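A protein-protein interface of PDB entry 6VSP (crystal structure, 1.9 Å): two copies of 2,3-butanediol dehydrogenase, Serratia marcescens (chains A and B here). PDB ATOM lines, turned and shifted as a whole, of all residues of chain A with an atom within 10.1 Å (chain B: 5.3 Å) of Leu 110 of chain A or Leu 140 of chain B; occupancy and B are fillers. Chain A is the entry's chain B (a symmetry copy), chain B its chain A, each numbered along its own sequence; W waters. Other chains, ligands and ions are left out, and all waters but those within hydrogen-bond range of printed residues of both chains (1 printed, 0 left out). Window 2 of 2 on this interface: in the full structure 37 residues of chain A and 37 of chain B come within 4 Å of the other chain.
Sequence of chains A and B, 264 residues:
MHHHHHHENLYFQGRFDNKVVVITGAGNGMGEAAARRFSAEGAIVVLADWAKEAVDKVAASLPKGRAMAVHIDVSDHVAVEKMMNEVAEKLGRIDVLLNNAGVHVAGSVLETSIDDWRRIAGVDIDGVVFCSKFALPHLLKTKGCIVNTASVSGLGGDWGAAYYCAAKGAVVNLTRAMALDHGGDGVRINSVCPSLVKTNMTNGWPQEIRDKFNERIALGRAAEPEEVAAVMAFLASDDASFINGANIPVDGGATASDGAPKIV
NZ of Lys 133 of chain B sits at hydrogen-bond distance from O of Val 109 of chain A, 2.7 Å away.
O of Thr 112 of chain A sits at hydrogen-bond distance from NZ of Lys 133 of chain B (2.9 Å).
The backbone carbonyl oxygen (O) of His 182 of chain B lies within hydrogen-bond range of the backbone NH (N) of Val 187 of chain B (3.2 Å).
The side-chain hydroxyl (OG) of Ser 108 of chain A sits close to the backbone NH (N) of Leu 110 of chain A (3.1 Å).
N of Ser 108 of chain A is in hydrogen-bond range of OE1 of Glu 111 of chain A (2.8 Å).
The backbone carbonyl oxygen (O) of Ser 108 of chain A sits at hydrogen-bond distance from the side-chain hydroxyl (OG1) of Thr 112 of chain A (2.7 Å).
The side-chain hydroxyl of Tyr 163 of chain A is in hydrogen-bond range of the backbone carbonyl oxygen of Thr 112 of chain A, at 2.9 Å.
CB of Ser 108 of chain A touches CE1 of His 182 of chain B, at 3.8 Å.
Lys 133 of chain B touches Leu 110 of chain A.
Leu 136 of chain B touches Leu 110 of chain A (CD2 to CG, 3.6 Å).
CD1 of Leu 110 of chain A touches CD1 of Leu 140 of chain B (3.8 Å).
His 182 of chain B touches Leu 110 of chain A.
Lys 133 of chain B touches Tyr 163 of chain A (CD to OH, 3.6 Å).
Of the printed residues of chain B, Ser 108 of chain A touches His 182.
Of the printed residues of chain B, Val 109 of chain A touches Lys 133.
Leu 110 of chain A touches just these residues of chain B: Lys 133, Leu 136, Leu 140 and His 182.
Of the printed residues of chain B, Tyr 163 of chain A touches Lys 133.
Printed residues of chain A within 4 Å of Lys 133 of chain B: Val 109, Leu 110, Thr 112 and Tyr 163.
Leu 136 of chain B touches just one residue of chain A: Leu 110 (3.6 Å).
No residue of chain A comes within 4 Å of Pro 137 of chain B.
No residue of chain A comes within 4 Å of Leu 139 of chain B.
Of chain A, only Leu 110 comes within 4 Å of Leu 140 of chain B.
Of the printed residues of chain A, His 182 of chain B touches Ser 108 (3.8 Å) and Leu 110 (3.9 Å).
No residue of chain A comes within 4 Å of Asp 185 of chain B.
The nearest residue of chain B that does not touch Leu 110 of chain A is Pro 137 of chain B (4.3 Å).
Of the 14 printed residues of chain B, 4 touch a printed residue of chain A.
Hydrophobic or aromatic side chains of chain B within 4 Å of the printed part of chain A: Leu 136, Leu 140 and His 182.
Hydrophobic or aromatic side chains of chain A within 4 Å of the printed part of chain B: Leu 110 and Tyr 163.
Among the printed residues, no Asp or Glu carboxylate lies within 4 Å of a Lys or Arg side-chain nitrogen of the other chain.
No position is printed for both chains.
Of the 8 pairs that touch across the chains among the printed residues, none has its exchanged pair printed and touching as well.
Water W1 lies within hydrogen-bond range of NE2 of His 182 of chain B (2.9 Å) and N of Val 109 of chain A (2.9 Å).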
ATOM      1  N   VAL A 105       9.852   4.289  36.075  1.00  0.00           N
ATOM      2  CA  VAL A 105      10.242   3.719  34.756  1.00  0.00           C
ATOM      3  C   VAL A 105      11.645   3.170  34.946  1.00  0.00           C
ATOM      4  O   VAL A 105      12.459   3.932  35.508  1.00  0.00           O
ATOM      5  CB  VAL A 105      10.228   4.755  33.627  1.00  0.00           C
ATOM      6  CG1 VAL A 105      10.593   4.095  32.310  1.00  0.00           C
ATOM      7  CG2 VAL A 105       8.902   5.486  33.512  1.00  0.00           C
ATOM      8  N   ALA A 106      11.924   1.952  34.466  1.00  0.00           N
ATOM      9  CA  ALA A 106      13.237   1.307  34.612  1.00  0.00           C
ATOM     10  C   ALA A 106      14.140   1.717  33.440  1.00  0.00           C
ATOM     11  O   ALA A 106      13.638   1.887  32.299  1.00  0.00           O
ATOM     12  CB  ALA A 106      13.085  -0.190  34.736  1.00  0.00           C
ATOM     13  N   GLY A 107      15.422   1.929  33.730  1.00  0.00           N
ATOM     14  CA  GLY A 107      16.455   2.070  32.691  1.00  0.00           C
ATOM     15  C   GLY A 107      17.439   3.178  33.015  1.00  0.00           C
ATOM     16  O   GLY A 107      17.095   4.083  33.826  1.00  0.00           O
ATOM     17  N   SER A 108      18.630   3.096  32.426  1.00  0.00           N
ATOM     18  CA  SER A 108      19.613   4.210  32.374  1.00  0.00           C
ATOM     19  C   SER A 108      19.022   5.310  31.492  1.00  0.00           C
ATOM     20  O   SER A 108      17.972   5.046  30.839  1.00  0.00           O
ATOM     21  CB  SER A 108      20.923   3.712  31.858  1.00  0.00           C
ATOM     22  OG  SER A 108      20.812   3.497  30.459  1.00  0.00           O
ATOM     23  N   VAL A 109      19.624   6.492  31.446  1.00  0.00           N
ATOM     24  CA  VAL A 109      19.179   7.570  30.503  1.00  0.00           C
ATOM     25  C   VAL A 109      19.314   7.076  29.051  1.00  0.00           C
ATOM     26  O   VAL A 109      18.682   7.697  28.185  1.00  0.00           O
ATOM     27  CB  VAL A 109      19.951   8.892  30.694  1.00  0.00           C
ATOM     28  CG1 VAL A 109      19.903   9.379  32.144  1.00  0.00           C
ATOM     29  CG2 VAL A 109      21.408   8.759  30.242  1.00  0.00           C
ATOM     30  N   LEU A 110      20.141   6.062  28.774  1.00  0.00           N
ATOM     31  CA  LEU A 110      20.316   5.538  27.383  1.00  0.00           C
ATOM     32  C   LEU A 110      19.138   4.631  27.007  1.00  0.00           C
ATOM     33  O   LEU A 110      18.875   4.480  25.795  1.00  0.00           O
ATOM     34  CB  LEU A 110      21.641   4.783  27.245  1.00  0.00           C
ATOM     35  CG  LEU A 110      22.903   5.644  27.379  1.00  0.00           C
ATOM     36  CD1 LEU A 110      24.154   4.814  27.141  1.00  0.00           C
ATOM     37  CD2 LEU A 110      22.878   6.840  26.440  1.00  0.00           C
ATOM     38  N   GLU A 111      18.445   4.078  27.998  1.00  0.00           N
ATOM     39  CA  GLU A 111      17.345   3.100  27.797  1.00  0.00           C
ATOM     40  C   GLU A 111      15.992   3.787  27.996  1.00  0.00           C
ATOM     41  O   GLU A 111      14.997   3.102  27.883  1.00  0.00           O
ATOM     42  CB  GLU A 111      17.475   1.914  28.758  1.00  0.00           C
ATOM     43  CG  GLU A 111      18.773   1.133  28.640  1.00  0.00           C
ATOM     44  CD  GLU A 111      19.080   0.249  29.834  1.00  0.00           C
ATOM     45  OE1 GLU A 111      18.791   0.663  30.979  1.00  0.00           O
ATOM     46  OE2 GLU A 111      19.612  -0.865  29.631  1.00  0.00           O
ATOM     47  N   THR A 112      15.949   5.079  28.326  1.00  0.00           N
ATOM     48  CA  THR A 112      14.692   5.772  28.686  1.00  0.00           C
ATOM     49  C   THR A 112      14.631   7.067  27.906  1.00  0.00           C
ATOM     50  O   THR A 112      15.685   7.666  27.722  1.00  0.00           O
ATOM     51  CB  THR A 112      14.569   5.979  30.201  1.00  0.00           C
ATOM     52  OG1 THR A 112      15.776   6.530  30.737  1.00  0.00           O
ATOM     53  CG2 THR A 112      14.268   4.690  30.916  1.00  0.00           C
ATOM     54  N   SER A 113      13.426   7.443  27.465  1.00  0.00           N
ATOM     55  CA  SER A 113      13.158   8.501  26.473  1.00  0.00           C
ATOM     56  C   SER A 113      12.901   9.839  27.164  1.00  0.00           C
ATOM     57  O   SER A 113      12.725   9.841  28.383  1.00  0.00           O
ATOM     58  CB  SER A 113      11.979   8.106  25.624  1.00  0.00           C
ATOM     59  OG  SER A 113      10.829   7.968  26.441  1.00  0.00           O
ATOM     60  N   ILE A 114      12.809  10.913  26.386  1.00  0.00           N
ATOM     61  CA  ILE A 114      12.349  12.246  26.843  1.00  0.00           C
ATOM     62  C   ILE A 114      10.964  12.068  27.467  1.00  0.00           C
ATOM     63  O   ILE A 114      10.707  12.667  28.523  1.00  0.00           O
ATOM     64  CB  ILE A 114      12.321  13.272  25.697  1.00  0.00           C
ATOM     65  CG1 ILE A 114      13.674  13.430  24.995  1.00  0.00           C
ATOM     66  CG2 ILE A 114      11.810  14.614  26.189  1.00  0.00           C
ATOM     67  CD1 ILE A 114      14.840  13.717  25.916  1.00  0.00           C
ATOM     68  N   ASP A 116       9.703   9.387  28.862  1.00  0.00           N
ATOM     69  CA  ASP A 116       9.885   8.729  30.177  1.00  0.00           C
ATOM     70  C   ASP A 116      10.288   9.805  31.202  1.00  0.00           C
ATOM     71  O   ASP A 116       9.771   9.774  32.323  1.00  0.00           O
ATOM     72  CB  ASP A 116      10.889   7.593  30.098  1.00  0.00           C
ATOM     73  CG  ASP A 116      10.422   6.385  29.287  1.00  0.00           C
ATOM     74  OD1 ASP A 116       9.189   6.105  29.268  1.00  0.00           O
ATOM     75  OD2 ASP A 116      11.303   5.721  28.695  1.00  0.00           O
ATOM     76  N   GLY A 160      19.939   1.401  36.912  1.00  0.00           N
ATOM     77  CA  GLY A 160      18.830   1.186  35.959  1.00  0.00           C
ATOM     78  C   GLY A 160      17.552   1.897  36.361  1.00  0.00           C
ATOM     79  O   GLY A 160      16.459   1.348  36.084  1.00  0.00           O
ATOM     80  N   ALA A 161      17.652   3.106  36.940  1.00  0.00           N
ATOM     81  CA  ALA A 161      16.475   3.971  37.231  1.00  0.00           C
ATOM     82  C   ALA A 161      16.916   5.439  37.340  1.00  0.00           C
ATOM     83  O   ALA A 161      16.622   6.091  38.362  1.00  0.00           O
ATOM     84  CB  ALA A 161      15.789   3.467  38.487  1.00  0.00           C
ATOM     85  N   ALA A 162      17.591   5.950  36.314  1.00  0.00           N
ATOM     86  CA  ALA A 162      18.330   7.239  36.403  1.00  0.00           C
ATOM     87  C   ALA A 162      17.343   8.393  36.618  1.00  0.00           C
ATOM     88  O   ALA A 162      17.523   9.197  37.585  1.00  0.00           O
ATOM     89  CB  ALA A 162      19.166   7.436  35.172  1.00  0.00           C
ATOM     90  N   TYR A 163      16.341   8.511  35.751  1.00  0.00           N
ATOM     91  CA  TYR A 163      15.319   9.587  35.855  1.00  0.00           C
ATOM     92  C   TYR A 163      14.597   9.502  37.203  1.00  0.00           C
ATOM     93  O   TYR A 163      14.407  10.545  37.815  1.00  0.00           O
ATOM     94  CB  TYR A 163      14.262   9.506  34.757  1.00  0.00           C
ATOM     95  CG  TYR A 163      14.766   9.672  33.347  1.00  0.00           C
ATOM     96  CD1 TYR A 163      15.976  10.291  33.059  1.00  0.00           C
ATOM     97  CD2 TYR A 163      14.032   9.160  32.288  1.00  0.00           C
ATOM     98  CE1 TYR A 163      16.427  10.413  31.758  1.00  0.00           C
ATOM     99  CE2 TYR A 163      14.469   9.291  30.984  1.00  0.00           C
ATOM    100  CZ  TYR A 163      15.671   9.915  30.711  1.00  0.00           C
ATOM    101  OH  TYR A 163      16.128  10.030  29.427  1.00  0.00           O
ATOM    102  N   LYS B 133      22.558  12.838  28.472  1.00  0.00           N
ATOM    103  CA  LYS B 133      21.948  11.764  27.638  1.00  0.00           C
ATOM    104  C   LYS B 133      22.588  11.794  26.232  1.00  0.00           C
ATOM    105  O   LYS B 133      23.029  10.735  25.752  1.00  0.00           O
ATOM    106  CB  LYS B 133      20.424  11.941  27.588  1.00  0.00           C
ATOM    107  CG  LYS B 133      19.669  10.947  26.700  1.00  0.00           C
ATOM    108  CD  LYS B 133      18.163  11.175  26.654  1.00  0.00           C
ATOM    109  CE  LYS B 133      17.444  10.259  25.668  1.00  0.00           C
ATOM    110  NZ  LYS B 133      17.669   8.831  25.978  1.00  0.00           N
ATOM    111  N   ALA B 135      25.413  13.475  25.155  1.00  0.00           N
ATOM    112  CA  ALA B 135      26.893  13.370  25.102  1.00  0.00           C
ATOM    113  C   ALA B 135      27.331  11.924  25.350  1.00  0.00           C
ATOM    114  O   ALA B 135      28.407  11.556  24.873  1.00  0.00           O
ATOM    115  CB  ALA B 135      27.557  14.308  26.084  1.00  0.00           C
ATOM    116  N   LEU B 136      26.551  11.134  26.094  1.00  0.00           N
ATOM    117  CA  LEU B 136      27.053   9.869  26.677  1.00  0.00           C
ATOM    118  C   LEU B 136      27.538   8.917  25.573  1.00  0.00           C
ATOM    119  O   LEU B 136      28.562   8.257  25.733  1.00  0.00           O
ATOM    120  CB  LEU B 136      25.962   9.251  27.549  1.00  0.00           C
ATOM    121  CG  LEU B 136      26.372   8.090  28.445  1.00  0.00           C
ATOM    122  CD1 LEU B 136      27.551   8.409  29.340  1.00  0.00           C
ATOM    123  CD2 LEU B 136      25.194   7.652  29.293  1.00  0.00           C
ATOM    124  N   PRO B 137      26.815   8.742  24.443  1.00  0.00           N
ATOM    125  CA  PRO B 137      27.275   7.790  23.421  1.00  0.00           C
ATOM    126  C   PRO B 137      28.701   8.120  22.940  1.00  0.00           C
ATOM    127  O   PRO B 137      29.492   7.212  22.723  1.00  0.00           O
ATOM    128  CB  PRO B 137      26.226   7.910  22.300  1.00  0.00           C
ATOM    129  CG  PRO B 137      24.991   8.476  22.987  1.00  0.00           C
ATOM    130  CD  PRO B 137      25.525   9.371  24.094  1.00  0.00           C
ATOM    131  N   HIS B 138      29.021   9.407  22.841  1.00  0.00           N
ATOM    132  CA  HIS B 138      30.354   9.931  22.445  1.00  0.00           C
ATOM    133  C   HIS B 138      31.369   9.706  23.573  1.00  0.00           C
ATOM    134  O   HIS B 138      32.495   9.219  23.296  1.00  0.00           O
ATOM    135  CB  HIS B 138      30.217  11.389  22.007  1.00  0.00           C
ATOM    136  CG  HIS B 138      29.193  11.586  20.948  1.00  0.00           C
ATOM    137  ND1 HIS B 138      29.295  10.972  19.708  1.00  0.00           N
ATOM    138  CD2 HIS B 138      28.042  12.291  20.937  1.00  0.00           C
ATOM    139  CE1 HIS B 138      28.253  11.308  18.976  1.00  0.00           C
ATOM    140  NE2 HIS B 138      27.472  12.140  19.687  1.00  0.00           N
ATOM    141  N   LEU B 139      30.991  10.003  24.824  1.00  0.00           N
ATOM    142  CA  LEU B 139      31.885   9.781  26.000  1.00  0.00           C
ATOM    143  C   LEU B 139      32.193   8.288  26.109  1.00  0.00           C
ATOM    144  O   LEU B 139      33.309   7.933  26.511  1.00  0.00           O
ATOM    145  CB  LEU B 139      31.212  10.304  27.277  1.00  0.00           C
ATOM    146  CG  LEU B 139      30.938  11.805  27.316  1.00  0.00           C
ATOM    147  CD1 LEU B 139      30.024  12.149  28.488  1.00  0.00           C
ATOM    148  CD2 LEU B 139      32.248  12.581  27.427  1.00  0.00           C
ATOM    149  N   LEU B 140      31.247   7.410  25.788  1.00  0.00           N
ATOM    150  CA  LEU B 140      31.504   5.948  25.910  1.00  0.00           C
ATOM    151  C   LEU B 140      32.654   5.542  24.975  1.00  0.00           C
ATOM    152  O   LEU B 140      33.498   4.685  25.399  1.00  0.00           O
ATOM    153  CB  LEU B 140      30.212   5.192  25.611  1.00  0.00           C
ATOM    154  CG  LEU B 140      29.258   5.100  26.796  1.00  0.00           C
ATOM    155  CD1 LEU B 140      27.851   4.754  26.324  1.00  0.00           C
ATOM    156  CD2 LEU B 140      29.772   4.092  27.799  1.00  0.00           C
ATOM    157  N   LYS B 141      32.736   6.181  23.809  1.00  0.00           N
ATOM    158  CA  LYS B 141      33.782   5.878  22.783  1.00  0.00           C
ATOM    159  C   LYS B 141      35.158   6.332  23.280  1.00  0.00           C
ATOM    160  O   LYS B 141      36.131   5.643  22.976  1.00  0.00           O
ATOM    161  CB  LYS B 141      33.457   6.530  21.437  1.00  0.00           C
ATOM    162  CG  LYS B 141      32.305   5.886  20.682  1.00  0.00           C
ATOM    163  CD  LYS B 141      31.846   6.679  19.471  1.00  0.00           C
ATOM    164  CE  LYS B 141      30.512   6.195  18.931  1.00  0.00           C
ATOM    165  NZ  LYS B 141      29.833   7.223  18.100  1.00  0.00           N
ATOM    166  N   THR B 142      35.237   7.410  24.070  1.00  0.00           N
ATOM    167  CA  THR B 142      36.530   7.957  24.575  1.00  0.00           C
ATOM    168  C   THR B 142      36.823   7.510  26.017  1.00  0.00           C
ATOM    169  O   THR B 142      37.902   7.842  26.525  1.00  0.00           O
ATOM    170  CB  THR B 142      36.538   9.483  24.462  1.00  0.00           C
ATOM    171  OG1 THR B 142      35.419  10.008  25.185  1.00  0.00           O
ATOM    172  CG2 THR B 142      36.494   9.948  23.020  1.00  0.00           C
ATOM    173  N   LYS B 143      35.917   6.781  26.676  1.00  0.00           N
ATOM    174  CA  LYS B 143      35.995   6.539  28.135  1.00  0.00           C
ATOM    175  C   LYS B 143      36.199   7.903  28.809  1.00  0.00           C
ATOM    176  O   LYS B 143      37.074   8.041  29.693  1.00  0.00           O
ATOM    177  CB  LYS B 143      37.063   5.487  28.439  1.00  0.00           C
ATOM    178  CG  LYS B 143      36.886   4.200  27.636  1.00  0.00           C
ATOM    179  CD  LYS B 143      37.217   2.918  28.350  1.00  0.00           C
ATOM    180  CE  LYS B 143      36.618   1.711  27.648  1.00  0.00           C
ATOM    181  NZ  LYS B 143      36.425   0.572  28.583  1.00  0.00           N
ATOM    182  N   GLY B 144      35.368   8.852  28.390  1.00  0.00           N
ATOM    183  CA  GLY B 144      35.301  10.237  28.894  1.00  0.00           C
ATOM    184  C   GLY B 144      34.603  10.318  30.241  1.00  0.00           C
ATOM    185  O   GLY B 144      34.379   9.256  30.906  1.00  0.00           O
ATOM    186  N   HIS B 182      27.021   3.789  34.298  1.00  0.00           N
ATOM    187  CA  HIS B 182      27.989   3.983  33.187  1.00  0.00           C
ATOM    188  C   HIS B 182      29.436   3.833  33.639  1.00  0.00           C
ATOM    189  O   HIS B 182      30.295   3.699  32.753  1.00  0.00           O
ATOM    190  CB  HIS B 182      27.726   5.301  32.473  1.00  0.00           C
ATOM    191  CG  HIS B 182      26.311   5.420  32.045  1.00  0.00           C
ATOM    192  ND1 HIS B 182      25.743   4.528  31.150  1.00  0.00           N
ATOM    193  CD2 HIS B 182      25.330   6.259  32.448  1.00  0.00           C
ATOM    194  CE1 HIS B 182      24.464   4.838  31.007  1.00  0.00           C
ATOM    195  NE2 HIS B 182      24.187   5.900  31.792  1.00  0.00           N
ATOM    196  N   ASP B 185      31.290   0.926  32.177  1.00  0.00           N
ATOM    197  CA  ASP B 185      31.554   1.073  30.722  1.00  0.00           C
ATOM    198  C   ASP B 185      32.636   2.149  30.510  1.00  0.00           C
ATOM    199  O   ASP B 185      32.792   2.610  29.346  1.00  0.00           O
ATOM    200  CB  ASP B 185      30.241   1.385  29.996  1.00  0.00           C
ATOM    201  CG  ASP B 185      29.188   0.305  30.200  1.00  0.00           C
ATOM    202  OD1 ASP B 185      29.574  -0.884  30.121  1.00  0.00           O
ATOM    203  OD2 ASP B 185      28.009   0.653  30.517  1.00  0.00           O
ATOM    204  N   VAL B 187      32.935   5.364  31.875  1.00  0.00           N
ATOM    205  CA  VAL B 187      32.551   6.802  31.929  1.00  0.00           C
ATOM    206  C   VAL B 187      32.253   7.144  33.396  1.00  0.00           C
ATOM    207  O   VAL B 187      31.221   6.699  33.940  1.00  0.00           O
ATOM    208  CB  VAL B 187      31.373   7.126  30.991  1.00  0.00           C
ATOM    209  CG1 VAL B 187      30.833   8.535  31.206  1.00  0.00           C
ATOM    210  CG2 VAL B 187      31.750   6.878  29.519  1.00  0.00           C
HETATM  211  O   HOH W   1      21.854   6.649  33.327  1.00  0.00           O
